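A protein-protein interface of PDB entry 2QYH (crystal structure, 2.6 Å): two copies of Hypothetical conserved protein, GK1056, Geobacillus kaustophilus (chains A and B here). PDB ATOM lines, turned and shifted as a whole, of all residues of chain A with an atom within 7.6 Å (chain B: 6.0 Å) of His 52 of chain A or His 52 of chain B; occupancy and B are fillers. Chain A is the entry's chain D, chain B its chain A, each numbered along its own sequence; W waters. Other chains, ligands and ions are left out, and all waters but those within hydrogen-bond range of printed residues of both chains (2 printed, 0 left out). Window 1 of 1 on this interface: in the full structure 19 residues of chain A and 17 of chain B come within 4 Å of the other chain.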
ATOM      1  N   LEU A  21     -19.386  -1.460  13.178  1.00  0.00           N
ATOM      2  CA  LEU A  21     -19.922  -0.620  12.121  1.00  0.00           C
ATOM      3  C   LEU A  21     -19.562  -1.196  10.756  1.00  0.00           C
ATOM      4  O   LEU A  21     -18.397  -1.209  10.360  1.00  0.00           O
ATOM      5  CB  LEU A  21     -19.363   0.787  12.267  1.00  0.00           C
ATOM      6  CG  LEU A  21     -19.841   1.781  11.225  1.00  0.00           C
ATOM      7  CD1 LEU A  21     -21.343   1.961  11.303  1.00  0.00           C
ATOM      8  CD2 LEU A  21     -19.152   3.080  11.477  1.00  0.00           C
ATOM      9  N   PRO A  47     -26.523  12.609  24.250  1.00  0.00           N
ATOM     10  CA  PRO A  47     -25.527  12.916  23.221  1.00  0.00           C
ATOM     11  C   PRO A  47     -24.150  12.286  23.487  1.00  0.00           C
ATOM     12  O   PRO A  47     -23.578  11.634  22.611  1.00  0.00           O
ATOM     13  CB  PRO A  47     -25.485  14.437  23.237  1.00  0.00           C
ATOM     14  CG  PRO A  47     -26.925  14.792  23.522  1.00  0.00           C
ATOM     15  CD  PRO A  47     -27.309  13.801  24.613  1.00  0.00           C
ATOM     16  N   PHE A  48     -23.632  12.462  24.700  1.00  0.00           N
ATOM     17  CA  PHE A  48     -22.323  11.927  25.051  1.00  0.00           C
ATOM     18  C   PHE A  48     -22.228  10.410  25.049  1.00  0.00           C
ATOM     19  O   PHE A  48     -21.142   9.857  25.211  1.00  0.00           O
ATOM     20  CB  PHE A  48     -21.862  12.455  26.419  1.00  0.00           C
ATOM     21  CG  PHE A  48     -22.712  12.006  27.576  1.00  0.00           C
ATOM     22  CD1 PHE A  48     -23.749  12.805  28.051  1.00  0.00           C
ATOM     23  CD2 PHE A  48     -22.476  10.780  28.195  1.00  0.00           C
ATOM     24  CE1 PHE A  48     -24.540  12.388  29.130  1.00  0.00           C
ATOM     25  CE2 PHE A  48     -23.263  10.353  29.275  1.00  0.00           C
ATOM     26  CZ  PHE A  48     -24.295  11.158  29.741  1.00  0.00           C
ATOM     27  N   MET A  49     -23.352   9.729  24.863  1.00  0.00           N
ATOM     28  CA  MET A  49     -23.351   8.271  24.855  1.00  0.00           C
ATOM     29  C   MET A  49     -23.189   7.669  23.468  1.00  0.00           C
ATOM     30  O   MET A  49     -23.219   6.446  23.316  1.00  0.00           O
ATOM     31  CB  MET A  49     -24.631   7.735  25.495  1.00  0.00           C
ATOM     32  CG  MET A  49     -24.583   7.663  27.008  1.00  0.00           C
ATOM     33  SD  MET A  49     -26.294   7.200  27.788  1.00  0.00           S
ATOM     34  CE  MET A  49     -26.534   5.419  27.059  1.00  0.00           C
ATOM     35  N   PHE A  50     -23.035   8.516  22.454  1.00  0.00           N
ATOM     36  CA  PHE A  50     -22.854   8.013  21.095  1.00  0.00           C
ATOM     37  C   PHE A  50     -22.120   9.008  20.204  1.00  0.00           C
ATOM     38  O   PHE A  50     -22.352   9.090  18.994  1.00  0.00           O
ATOM     39  CB  PHE A  50     -24.206   7.600  20.472  1.00  0.00           C
ATOM     40  CG  PHE A  50     -25.146   8.744  20.191  1.00  0.00           C
ATOM     41  CD1 PHE A  50     -25.294   9.235  18.893  1.00  0.00           C
ATOM     42  CD2 PHE A  50     -25.935   9.285  21.208  1.00  0.00           C
ATOM     43  CE1 PHE A  50     -26.218  10.242  18.606  1.00  0.00           C
ATOM     44  CE2 PHE A  50     -26.867  10.296  20.935  1.00  0.00           C
ATOM     45  CZ  PHE A  50     -27.008  10.775  19.625  1.00  0.00           C
ATOM     46  N   GLU A  51     -21.214   9.756  20.824  1.00  0.00           N
ATOM     47  CA  GLU A  51     -20.421  10.741  20.109  1.00  0.00           C
ATOM     48  C   GLU A  51     -19.372  10.049  19.236  1.00  0.00           C
ATOM     49  O   GLU A  51     -19.057  10.522  18.145  1.00  0.00           O
ATOM     50  CB  GLU A  51     -19.730  11.666  21.099  1.00  0.00           C
ATOM     51  CG  GLU A  51     -19.061  12.856  20.464  1.00  0.00           C
ATOM     52  CD  GLU A  51     -18.295  13.677  21.473  1.00  0.00           C
ATOM     53  OE1 GLU A  51     -18.844  13.951  22.566  1.00  0.00           O
ATOM     54  OE2 GLU A  51     -17.144  14.052  21.173  1.00  0.00           O
ATOM     55  N   HIS A  52     -18.827   8.934  19.715  1.00  0.00           N
ATOM     56  CA  HIS A  52     -17.825   8.213  18.945  1.00  0.00           C
ATOM     57  C   HIS A  52     -18.422   7.758  17.607  1.00  0.00           C
ATOM     58  O   HIS A  52     -17.799   7.917  16.549  1.00  0.00           O
ATOM     59  CB  HIS A  52     -17.303   7.002  19.730  1.00  0.00           C
ATOM     60  CG  HIS A  52     -16.220   6.245  19.019  1.00  0.00           C
ATOM     61  ND1 HIS A  52     -15.017   6.816  18.663  1.00  0.00           N
ATOM     62  CD2 HIS A  52     -16.169   4.962  18.579  1.00  0.00           C
ATOM     63  CE1 HIS A  52     -14.274   5.925  18.037  1.00  0.00           C
ATOM     64  NE2 HIS A  52     -14.948   4.792  17.970  1.00  0.00           N
ATOM     65  N   VAL A  53     -19.630   7.195  17.660  1.00  0.00           N
ATOM     66  CA  VAL A  53     -20.308   6.739  16.452  1.00  0.00           C
ATOM     67  C   VAL A  53     -20.516   7.919  15.504  1.00  0.00           C
ATOM     68  O   VAL A  53     -20.316   7.796  14.295  1.00  0.00           O
ATOM     69  CB  VAL A  53     -21.695   6.157  16.764  1.00  0.00           C
ATOM     70  CG1 VAL A  53     -22.161   5.304  15.609  1.00  0.00           C
ATOM     71  CG2 VAL A  53     -21.651   5.358  18.055  1.00  0.00           C
ATOM     72  N   ARG A  54     -20.932   9.053  16.066  1.00  0.00           N
ATOM     73  CA  ARG A  54     -21.176  10.257  15.283  1.00  0.00           C
ATOM     74  C   ARG A  54     -19.909  10.694  14.565  1.00  0.00           C
ATOM     75  O   ARG A  54     -19.940  11.042  13.380  1.00  0.00           O
ATOM     76  CB  ARG A  54     -21.677  11.401  16.173  1.00  0.00           C
ATOM     77  CG  ARG A  54     -23.070  11.209  16.741  1.00  0.00           C
ATOM     78  CD  ARG A  54     -23.751  12.561  16.966  1.00  0.00           C
ATOM     79  NE  ARG A  54     -22.996  13.434  17.864  1.00  0.00           N
ATOM     80  CZ  ARG A  54     -22.943  13.281  19.185  1.00  0.00           C
ATOM     81  NH1 ARG A  54     -23.608  12.287  19.769  1.00  0.00           N
ATOM     82  NH2 ARG A  54     -22.223  14.119  19.925  1.00  0.00           N
ATOM     83  N   LYS A  55     -18.794  10.680  15.284  1.00  0.00           N
ATOM     84  CA  LYS A  55     -17.528  11.071  14.692  1.00  0.00           C
ATOM     85  C   LYS A  55     -17.118  10.076  13.608  1.00  0.00           C
ATOM     86  O   LYS A  55     -16.573  10.461  12.572  1.00  0.00           O
ATOM     87  CB  LYS A  55     -16.449  11.200  15.778  1.00  0.00           C
ATOM     88  CG  LYS A  55     -16.561  12.517  16.545  1.00  0.00           C
ATOM     89  CD  LYS A  55     -15.360  12.834  17.446  1.00  0.00           C
ATOM     90  CE  LYS A  55     -15.434  12.130  18.803  1.00  0.00           C
ATOM     91  NZ  LYS A  55     -14.439  12.664  19.797  1.00  0.00           N
ATOM     92  N   GLN A  56     -17.408   8.801  13.836  1.00  0.00           N
ATOM     93  CA  GLN A  56     -17.072   7.767  12.876  1.00  0.00           C
ATOM     94  C   GLN A  56     -17.794   7.965  11.540  1.00  0.00           C
ATOM     95  O   GLN A  56     -17.196   7.817  10.471  1.00  0.00           O
ATOM     96  CB  GLN A  56     -17.417   6.387  13.446  1.00  0.00           C
ATOM     97  CG  GLN A  56     -16.371   5.795  14.362  1.00  0.00           C
ATOM     98  CD  GLN A  56     -16.822   4.481  14.968  1.00  0.00           C
ATOM     99  OE1 GLN A  56     -17.618   4.457  15.902  1.00  0.00           O
ATOM    100  NE2 GLN A  56     -16.323   3.376  14.428  1.00  0.00           N
ATOM    101  N   LEU A  57     -19.080   8.296  11.611  1.00  0.00           N
ATOM    102  CA  LEU A  57     -19.893   8.492  10.420  1.00  0.00           C
ATOM    103  C   LEU A  57     -20.035   9.953  10.004  1.00  0.00           C
ATOM    104  O   LEU A  57     -20.691  10.259   9.007  1.00  0.00           O
ATOM    105  CB  LEU A  57     -21.285   7.896  10.643  1.00  0.00           C
ATOM    106  CG  LEU A  57     -21.358   6.373  10.792  1.00  0.00           C
ATOM    107  CD1 LEU A  57     -22.775   5.945  11.143  1.00  0.00           C
ATOM    108  CD2 LEU A  57     -20.914   5.722   9.488  1.00  0.00           C
ATOM    109  N   GLY A  58     -19.425  10.855  10.764  1.00  0.00           N
ATOM    110  CA  GLY A  58     -19.533  12.263  10.448  1.00  0.00           C
ATOM    111  C   GLY A  58     -20.986  12.711  10.496  1.00  0.00           C
ATOM    112  O   GLY A  58     -21.444  13.472   9.643  1.00  0.00           O
ATOM    113  N   LYS A 127     -22.120   0.025  30.045  1.00  0.00           N
ATOM    114  CA  LYS A 127     -20.669   0.139  29.931  1.00  0.00           C
ATOM    115  C   LYS A 127     -20.161   1.468  30.464  1.00  0.00           C
ATOM    116  O   LYS A 127     -19.203   2.040  29.944  1.00  0.00           O
ATOM    117  CB  LYS A 127     -20.209  -0.068  28.483  1.00  0.00           C
ATOM    118  CG  LYS A 127     -20.441  -1.478  27.962  1.00  0.00           C
ATOM    119  CD  LYS A 127     -19.872  -2.518  28.926  1.00  0.00           C
ATOM    120  CE  LYS A 127     -20.093  -3.936  28.425  1.00  0.00           C
ATOM    121  NZ  LYS A 127     -19.364  -4.197  27.150  1.00  0.00           N
ATOM    122  N   PHE A 128     -20.814   1.947  31.517  1.00  0.00           N
ATOM    123  CA  PHE A 128     -20.429   3.194  32.159  1.00  0.00           C
ATOM    124  C   PHE A 128     -20.052   3.027  33.620  1.00  0.00           C
ATOM    125  O   PHE A 128     -20.556   2.138  34.321  1.00  0.00           O
ATOM    126  CB  PHE A 128     -21.546   4.227  32.037  1.00  0.00           C
ATOM    127  CG  PHE A 128     -21.494   5.015  30.777  1.00  0.00           C
ATOM    128  CD1 PHE A 128     -22.141   4.566  29.635  1.00  0.00           C
ATOM    129  CD2 PHE A 128     -20.781   6.210  30.731  1.00  0.00           C
ATOM    130  CE1 PHE A 128     -22.083   5.295  28.454  1.00  0.00           C
ATOM    131  CE2 PHE A 128     -20.713   6.948  29.555  1.00  0.00           C
ATOM    132  CZ  PHE A 128     -21.365   6.488  28.413  1.00  0.00           C
ATOM    133  N   LEU B  15      -9.830  -1.911  26.051  1.00  0.00           N
ATOM    134  CA  LEU B  15     -10.826  -2.434  25.121  1.00  0.00           C
ATOM    135  C   LEU B  15     -10.400  -3.799  24.589  1.00  0.00           C
ATOM    136  O   LEU B  15      -9.221  -4.026  24.315  1.00  0.00           O
ATOM    137  CB  LEU B  15     -11.007  -1.476  23.945  1.00  0.00           C
ATOM    138  CG  LEU B  15     -11.364  -0.029  24.280  1.00  0.00           C
ATOM    139  CD1 LEU B  15     -11.414   0.796  23.002  1.00  0.00           C
ATOM    140  CD2 LEU B  15     -12.697   0.016  24.992  1.00  0.00           C
ATOM    141  N   LYS B  19     -13.436  -3.937  20.436  1.00  0.00           N
ATOM    142  CA  LYS B  19     -13.413  -2.516  20.770  1.00  0.00           C
ATOM    143  C   LYS B  19     -14.403  -2.195  21.888  1.00  0.00           C
ATOM    144  O   LYS B  19     -14.769  -1.040  22.094  1.00  0.00           O
ATOM    145  CB  LYS B  19     -13.713  -1.670  19.530  1.00  0.00           C
ATOM    146  CG  LYS B  19     -12.537  -1.533  18.586  1.00  0.00           C
ATOM    147  CD  LYS B  19     -11.448  -0.668  19.211  1.00  0.00           C
ATOM    148  CE  LYS B  19     -10.224  -0.556  18.312  1.00  0.00           C
ATOM    149  NZ  LYS B  19      -9.536  -1.868  18.145  1.00  0.00           N
ATOM    150  N   ARG B  45      -2.746   7.084  20.641  1.00  0.00           N
ATOM    151  CA  ARG B  45      -3.956   7.661  20.065  1.00  0.00           C
ATOM    152  C   ARG B  45      -4.088   9.142  20.342  1.00  0.00           C
ATOM    153  O   ARG B  45      -3.551   9.657  21.320  1.00  0.00           O
ATOM    154  CB  ARG B  45      -5.212   6.982  20.612  1.00  0.00           C
ATOM    155  CG  ARG B  45      -5.468   5.576  20.141  1.00  0.00           C
ATOM    156  CD  ARG B  45      -6.911   5.221  20.463  1.00  0.00           C
ATOM    157  NE  ARG B  45      -7.284   3.864  20.070  1.00  0.00           N
ATOM    158  CZ  ARG B  45      -8.526   3.393  20.144  1.00  0.00           C
ATOM    159  NH1 ARG B  45      -9.509   4.168  20.590  1.00  0.00           N
ATOM    160  NH2 ARG B  45      -8.785   2.144  19.779  1.00  0.00           N
ATOM    161  N   PHE B  48      -9.141  12.938  20.746  1.00  0.00           N
ATOM    162  CA  PHE B  48     -10.494  12.714  20.243  1.00  0.00           C
ATOM    163  C   PHE B  48     -10.794  11.280  19.807  1.00  0.00           C
ATOM    164  O   PHE B  48     -11.949  10.940  19.551  1.00  0.00           O
ATOM    165  CB  PHE B  48     -10.821  13.682  19.101  1.00  0.00           C
ATOM    166  CG  PHE B  48      -9.952  13.517  17.884  1.00  0.00           C
ATOM    167  CD1 PHE B  48      -8.723  14.175  17.792  1.00  0.00           C
ATOM    168  CD2 PHE B  48     -10.362  12.703  16.828  1.00  0.00           C
ATOM    169  CE1 PHE B  48      -7.910  14.025  16.659  1.00  0.00           C
ATOM    170  CE2 PHE B  48      -9.562  12.544  15.694  1.00  0.00           C
ATOM    171  CZ  PHE B  48      -8.330  13.209  15.608  1.00  0.00           C
ATOM    172  N   MET B  49      -9.767  10.437  19.749  1.00  0.00           N
ATOM    173  CA  MET B  49      -9.944   9.050  19.333  1.00  0.00           C
ATOM    174  C   MET B  49     -10.313   8.088  20.452  1.00  0.00           C
ATOM    175  O   MET B  49     -10.685   6.944  20.184  1.00  0.00           O
ATOM    176  CB  MET B  49      -8.696   8.564  18.599  1.00  0.00           C
ATOM    177  CG  MET B  49      -8.519   9.222  17.237  1.00  0.00           C
ATOM    178  SD  MET B  49      -9.855   8.697  15.924  1.00  0.00           S
ATOM    179  CE  MET B  49     -11.434   9.544  16.644  1.00  0.00           C
ATOM    180  N   PHE B  50     -10.216   8.540  21.702  1.00  0.00           N
ATOM    181  CA  PHE B  50     -10.582   7.687  22.832  1.00  0.00           C
ATOM    182  C   PHE B  50     -11.358   8.460  23.902  1.00  0.00           C
ATOM    183  O   PHE B  50     -11.343   8.116  25.084  1.00  0.00           O
ATOM    184  CB  PHE B  50      -9.337   6.999  23.419  1.00  0.00           C
ATOM    185  CG  PHE B  50      -8.345   7.934  24.052  1.00  0.00           C
ATOM    186  CD1 PHE B  50      -8.332   8.120  25.437  1.00  0.00           C
ATOM    187  CD2 PHE B  50      -7.407   8.605  23.276  1.00  0.00           C
ATOM    188  CE1 PHE B  50      -7.395   8.960  26.043  1.00  0.00           C
ATOM    189  CE2 PHE B  50      -6.459   9.451  23.873  1.00  0.00           C
ATOM    190  CZ  PHE B  50      -6.456   9.626  25.264  1.00  0.00           C
ATOM    191  N   GLU B  51     -12.051   9.505  23.452  1.00  0.00           N
ATOM    192  CA  GLU B  51     -12.870  10.347  24.314  1.00  0.00           C
ATOM    193  C   GLU B  51     -13.992   9.486  24.885  1.00  0.00           C
ATOM    194  O   GLU B  51     -14.407   9.671  26.027  1.00  0.00           O
ATOM    195  CB  GLU B  51     -13.450  11.506  23.493  1.00  0.00           C
ATOM    196  CG  GLU B  51     -14.261  12.557  24.262  1.00  0.00           C
ATOM    197  CD  GLU B  51     -15.660  12.096  24.685  1.00  0.00           C
ATOM    198  OE1 GLU B  51     -16.311  11.326  23.936  1.00  0.00           O
ATOM    199  OE2 GLU B  51     -16.117  12.533  25.769  1.00  0.00           O
ATOM    200  N   HIS B  52     -14.484   8.535  24.097  1.00  0.00           N
ATOM    201  CA  HIS B  52     -15.548   7.678  24.589  1.00  0.00           C
ATOM    202  C   HIS B  52     -15.068   6.839  25.778  1.00  0.00           C
ATOM    203  O   HIS B  52     -15.778   6.706  26.774  1.00  0.00           O
ATOM    204  CB  HIS B  52     -16.103   6.771  23.475  1.00  0.00           C
ATOM    205  CG  HIS B  52     -15.091   5.847  22.867  1.00  0.00           C
ATOM    206  ND1 HIS B  52     -14.103   6.282  22.009  1.00  0.00           N
ATOM    207  CD2 HIS B  52     -14.928   4.508  22.978  1.00  0.00           C
ATOM    208  CE1 HIS B  52     -13.379   5.251  21.614  1.00  0.00           C
ATOM    209  NE2 HIS B  52     -13.861   4.161  22.189  1.00  0.00           N
ATOM    210  N   VAL B  53     -13.860   6.291  25.687  1.00  0.00           N
ATOM    211  CA  VAL B  53     -13.338   5.474  26.775  1.00  0.00           C
ATOM    212  C   VAL B  53     -13.165   6.312  28.035  1.00  0.00           C
ATOM    213  O   VAL B  53     -13.454   5.862  29.139  1.00  0.00           O
ATOM    214  CB  VAL B  53     -11.979   4.842  26.406  1.00  0.00           C
ATOM    215  CG1 VAL B  53     -11.505   3.951  27.541  1.00  0.00           C
ATOM    216  CG2 VAL B  53     -12.117   4.032  25.129  1.00  0.00           C
ATOM    217  N   ARG B  54     -12.693   7.536  27.849  1.00  0.00           N
ATOM    218  CA  ARG B  54     -12.484   8.457  28.945  1.00  0.00           C
ATOM    219  C   ARG B  54     -13.806   8.776  29.634  1.00  0.00           C
ATOM    220  O   ARG B  54     -13.901   8.795  30.861  1.00  0.00           O
ATOM    221  CB  ARG B  54     -11.874   9.738  28.407  1.00  0.00           C
ATOM    222  CG  ARG B  54     -10.433   9.941  28.759  1.00  0.00           C
ATOM    223  CD  ARG B  54      -9.990  11.298  28.284  1.00  0.00           C
ATOM    224  NE  ARG B  54      -9.692  11.245  26.867  1.00  0.00           N
ATOM    225  CZ  ARG B  54     -10.103  12.137  25.976  1.00  0.00           C
ATOM    226  NH1 ARG B  54     -10.843  13.171  26.344  1.00  0.00           N
ATOM    227  NH2 ARG B  54      -9.762  11.987  24.707  1.00  0.00           N
ATOM    228  N   LYS B  55     -14.831   9.027  28.831  1.00  0.00           N
ATOM    229  CA  LYS B  55     -16.144   9.357  29.350  1.00  0.00           C
ATOM    230  C   LYS B  55     -16.735   8.163  30.090  1.00  0.00           C
ATOM    231  O   LYS B  55     -17.378   8.317  31.125  1.00  0.00           O
ATOM    232  CB  LYS B  55     -17.062   9.756  28.198  1.00  0.00           C
ATOM    233  CG  LYS B  55     -18.348  10.412  28.625  1.00  0.00           C
ATOM    234  CD  LYS B  55     -18.078  11.791  29.181  1.00  0.00           C
ATOM    235  CE  LYS B  55     -19.373  12.511  29.484  1.00  0.00           C
ATOM    236  NZ  LYS B  55     -19.115  13.908  29.893  1.00  0.00           N
ATOM    237  N   GLN B  56     -16.514   6.970  29.552  1.00  0.00           N
ATOM    238  CA  GLN B  56     -17.031   5.757  30.165  1.00  0.00           C
ATOM    239  C   GLN B  56     -16.413   5.429  31.524  1.00  0.00           C
ATOM    240  O   GLN B  56     -17.118   5.031  32.454  1.00  0.00           O
ATOM    241  CB  GLN B  56     -16.829   4.574  29.218  1.00  0.00           C
ATOM    242  CG  GLN B  56     -17.857   4.485  28.102  1.00  0.00           C
ATOM    243  CD  GLN B  56     -17.513   3.418  27.083  1.00  0.00           C
ATOM    244  OE1 GLN B  56     -16.670   3.625  26.212  1.00  0.00           O
ATOM    245  NE2 GLN B  56     -18.153   2.262  27.200  1.00  0.00           N
ATOM    246  N   LEU B  57     -15.100   5.600  31.635  1.00  0.00           N
ATOM    247  CA  LEU B  57     -14.386   5.291  32.867  1.00  0.00           C
ATOM    248  C   LEU B  57     -14.163   6.503  33.754  1.00  0.00           C
ATOM    249  O   LEU B  57     -13.692   6.377  34.882  1.00  0.00           O
ATOM    250  CB  LEU B  57     -13.038   4.652  32.533  1.00  0.00           C
ATOM    251  CG  LEU B  57     -13.114   3.296  31.831  1.00  0.00           C
ATOM    252  CD1 LEU B  57     -11.751   2.889  31.327  1.00  0.00           C
ATOM    253  CD2 LEU B  57     -13.659   2.267  32.800  1.00  0.00           C
ATOM    254  N   PHE B 128     -13.786   4.520  10.059  1.00  0.00           N
ATOM    255  CA  PHE B 128     -13.954   5.971  10.044  1.00  0.00           C
ATOM    256  C   PHE B 128     -14.258   6.503   8.660  1.00  0.00           C
ATOM    257  O   PHE B 128     -13.781   5.965   7.651  1.00  0.00           O
ATOM    258  CB  PHE B 128     -12.714   6.671  10.594  1.00  0.00           C
ATOM    259  CG  PHE B 128     -12.776   6.913  12.055  1.00  0.00           C
ATOM    260  CD1 PHE B 128     -12.507   5.888  12.953  1.00  0.00           C
ATOM    261  CD2 PHE B 128     -13.154   8.157  12.540  1.00  0.00           C
ATOM    262  CE1 PHE B 128     -12.616   6.096  14.322  1.00  0.00           C
ATOM    263  CE2 PHE B 128     -13.269   8.380  13.903  1.00  0.00           C
ATOM    264  CZ  PHE B 128     -13.000   7.342  14.800  1.00  0.00           C
HETATM  265  O   HOH W   1     -16.159  10.629  21.430  1.00  0.00           O
HETATM  266  O   HOH W   2     -14.070   8.887  20.987  1.00  0.00           O
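The side-chain amino group of Lys 55 of chain A is in hydrogen-bond range of the backbone carbonyl oxygen of Phe 48 of chain B, at 3.0 Å. The backbone carbonyl oxygen (O) of Lys 127 of chain A is in hydrogen-bond range of the side-chain amide nitrogen (NE2) of Gln 56 of chain B, at 2.9 Å.
O of His 52 of chain B lies close to OE1 of Gln 56 of chain B (3.3 Å). NZ of Lys 55 of chain A lies within salt-bridge range of OE2 of Glu 51 of chain A (3.3 Å). NE2 of His 52 of chain A lies close to OE1 of Gln 56 of chain A.
Among the printed residues, pairs that only touch across the chains: Phe 48 of chain A with Lys 55 of chain B, Glu 51 of chain A with Glu 51 of chain B, His 52 of chain A with His 52 of chain B, His 52 of chain A with Phe 128 of chain B, Lys 55 of chain A with Glu 51 of chain B, Gln 56 of chain A with Phe 128 of chain B, Phe 128 of chain A with Lys 55 of chain B and Phe 128 of chain A with Gln 56 of chain B.
His 52 of chain B touches one residue of chain A. Of the printed residues of chain A, Gln 56 of chain B touches Lys 127 (2.9 Å) and Phe 128 (3.7 Å). Of the printed residues of chain A, Glu 51 of chain B touches Glu 51 (3.9 Å) and Lys 55 (3.997 Å). Printed residues of chain B within 4 Å of Gln 56 of chain A: Phe 128. The nearest printed residue of chain B that does not touch Phe 128 of chain A is His 52 of chain B (5.7 Å).
Hydrophobic or aromatic side chains of chain A that line the printed part of chain B: Phe 48, His 52 and Phe 128. Of the 14 printed residues of chain B, 6 touch a printed residue of chain A. Hydrophobic or aromatic side chains of chain B within 4 Å of the printed part of chain A: Phe 48, His 52 and Phe 128.
Phe 48 of chain A touches Lys 55 of chain B, and with the chains exchanged Lys 55 of chain A touches Phe 48 of chain B. His 52 of chain B touches its own counterpart, His 52 of chain A. His 52 of chain A touches Phe 128 of chain B, but with the chains exchanged Phe 128 of chain A does not touch His 52 of chain B (5.7 Å). Lys 55 of chain A touches Glu 51 of chain B, but with the chains exchanged Glu 51 of chain A does not touch Lys 55 of chain B (7.0 Å). Of the 10 pairs that touch across the chains among the printed residues, 6 have their exchanged pair printed and touching as well.
Water W1 lies within hydrogen-bond range of the side-chain carboxylate (OE1) of Glu 51 of chain B and the side-chain amino group (NZ) of Lys 55 of chain A. Water W2 lies within hydrogen-bond range of a ring nitrogen (ND1) of His 52 of chain B (2.8 Å), the backbone NH (N) of Glu 51 of chain B (3.2 Å), a ring nitrogen (ND1) of His 52 of chain A (3.3 Å) and the backbone carbonyl oxygen (O) of Phe 48 of chain B (3.3 Å).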
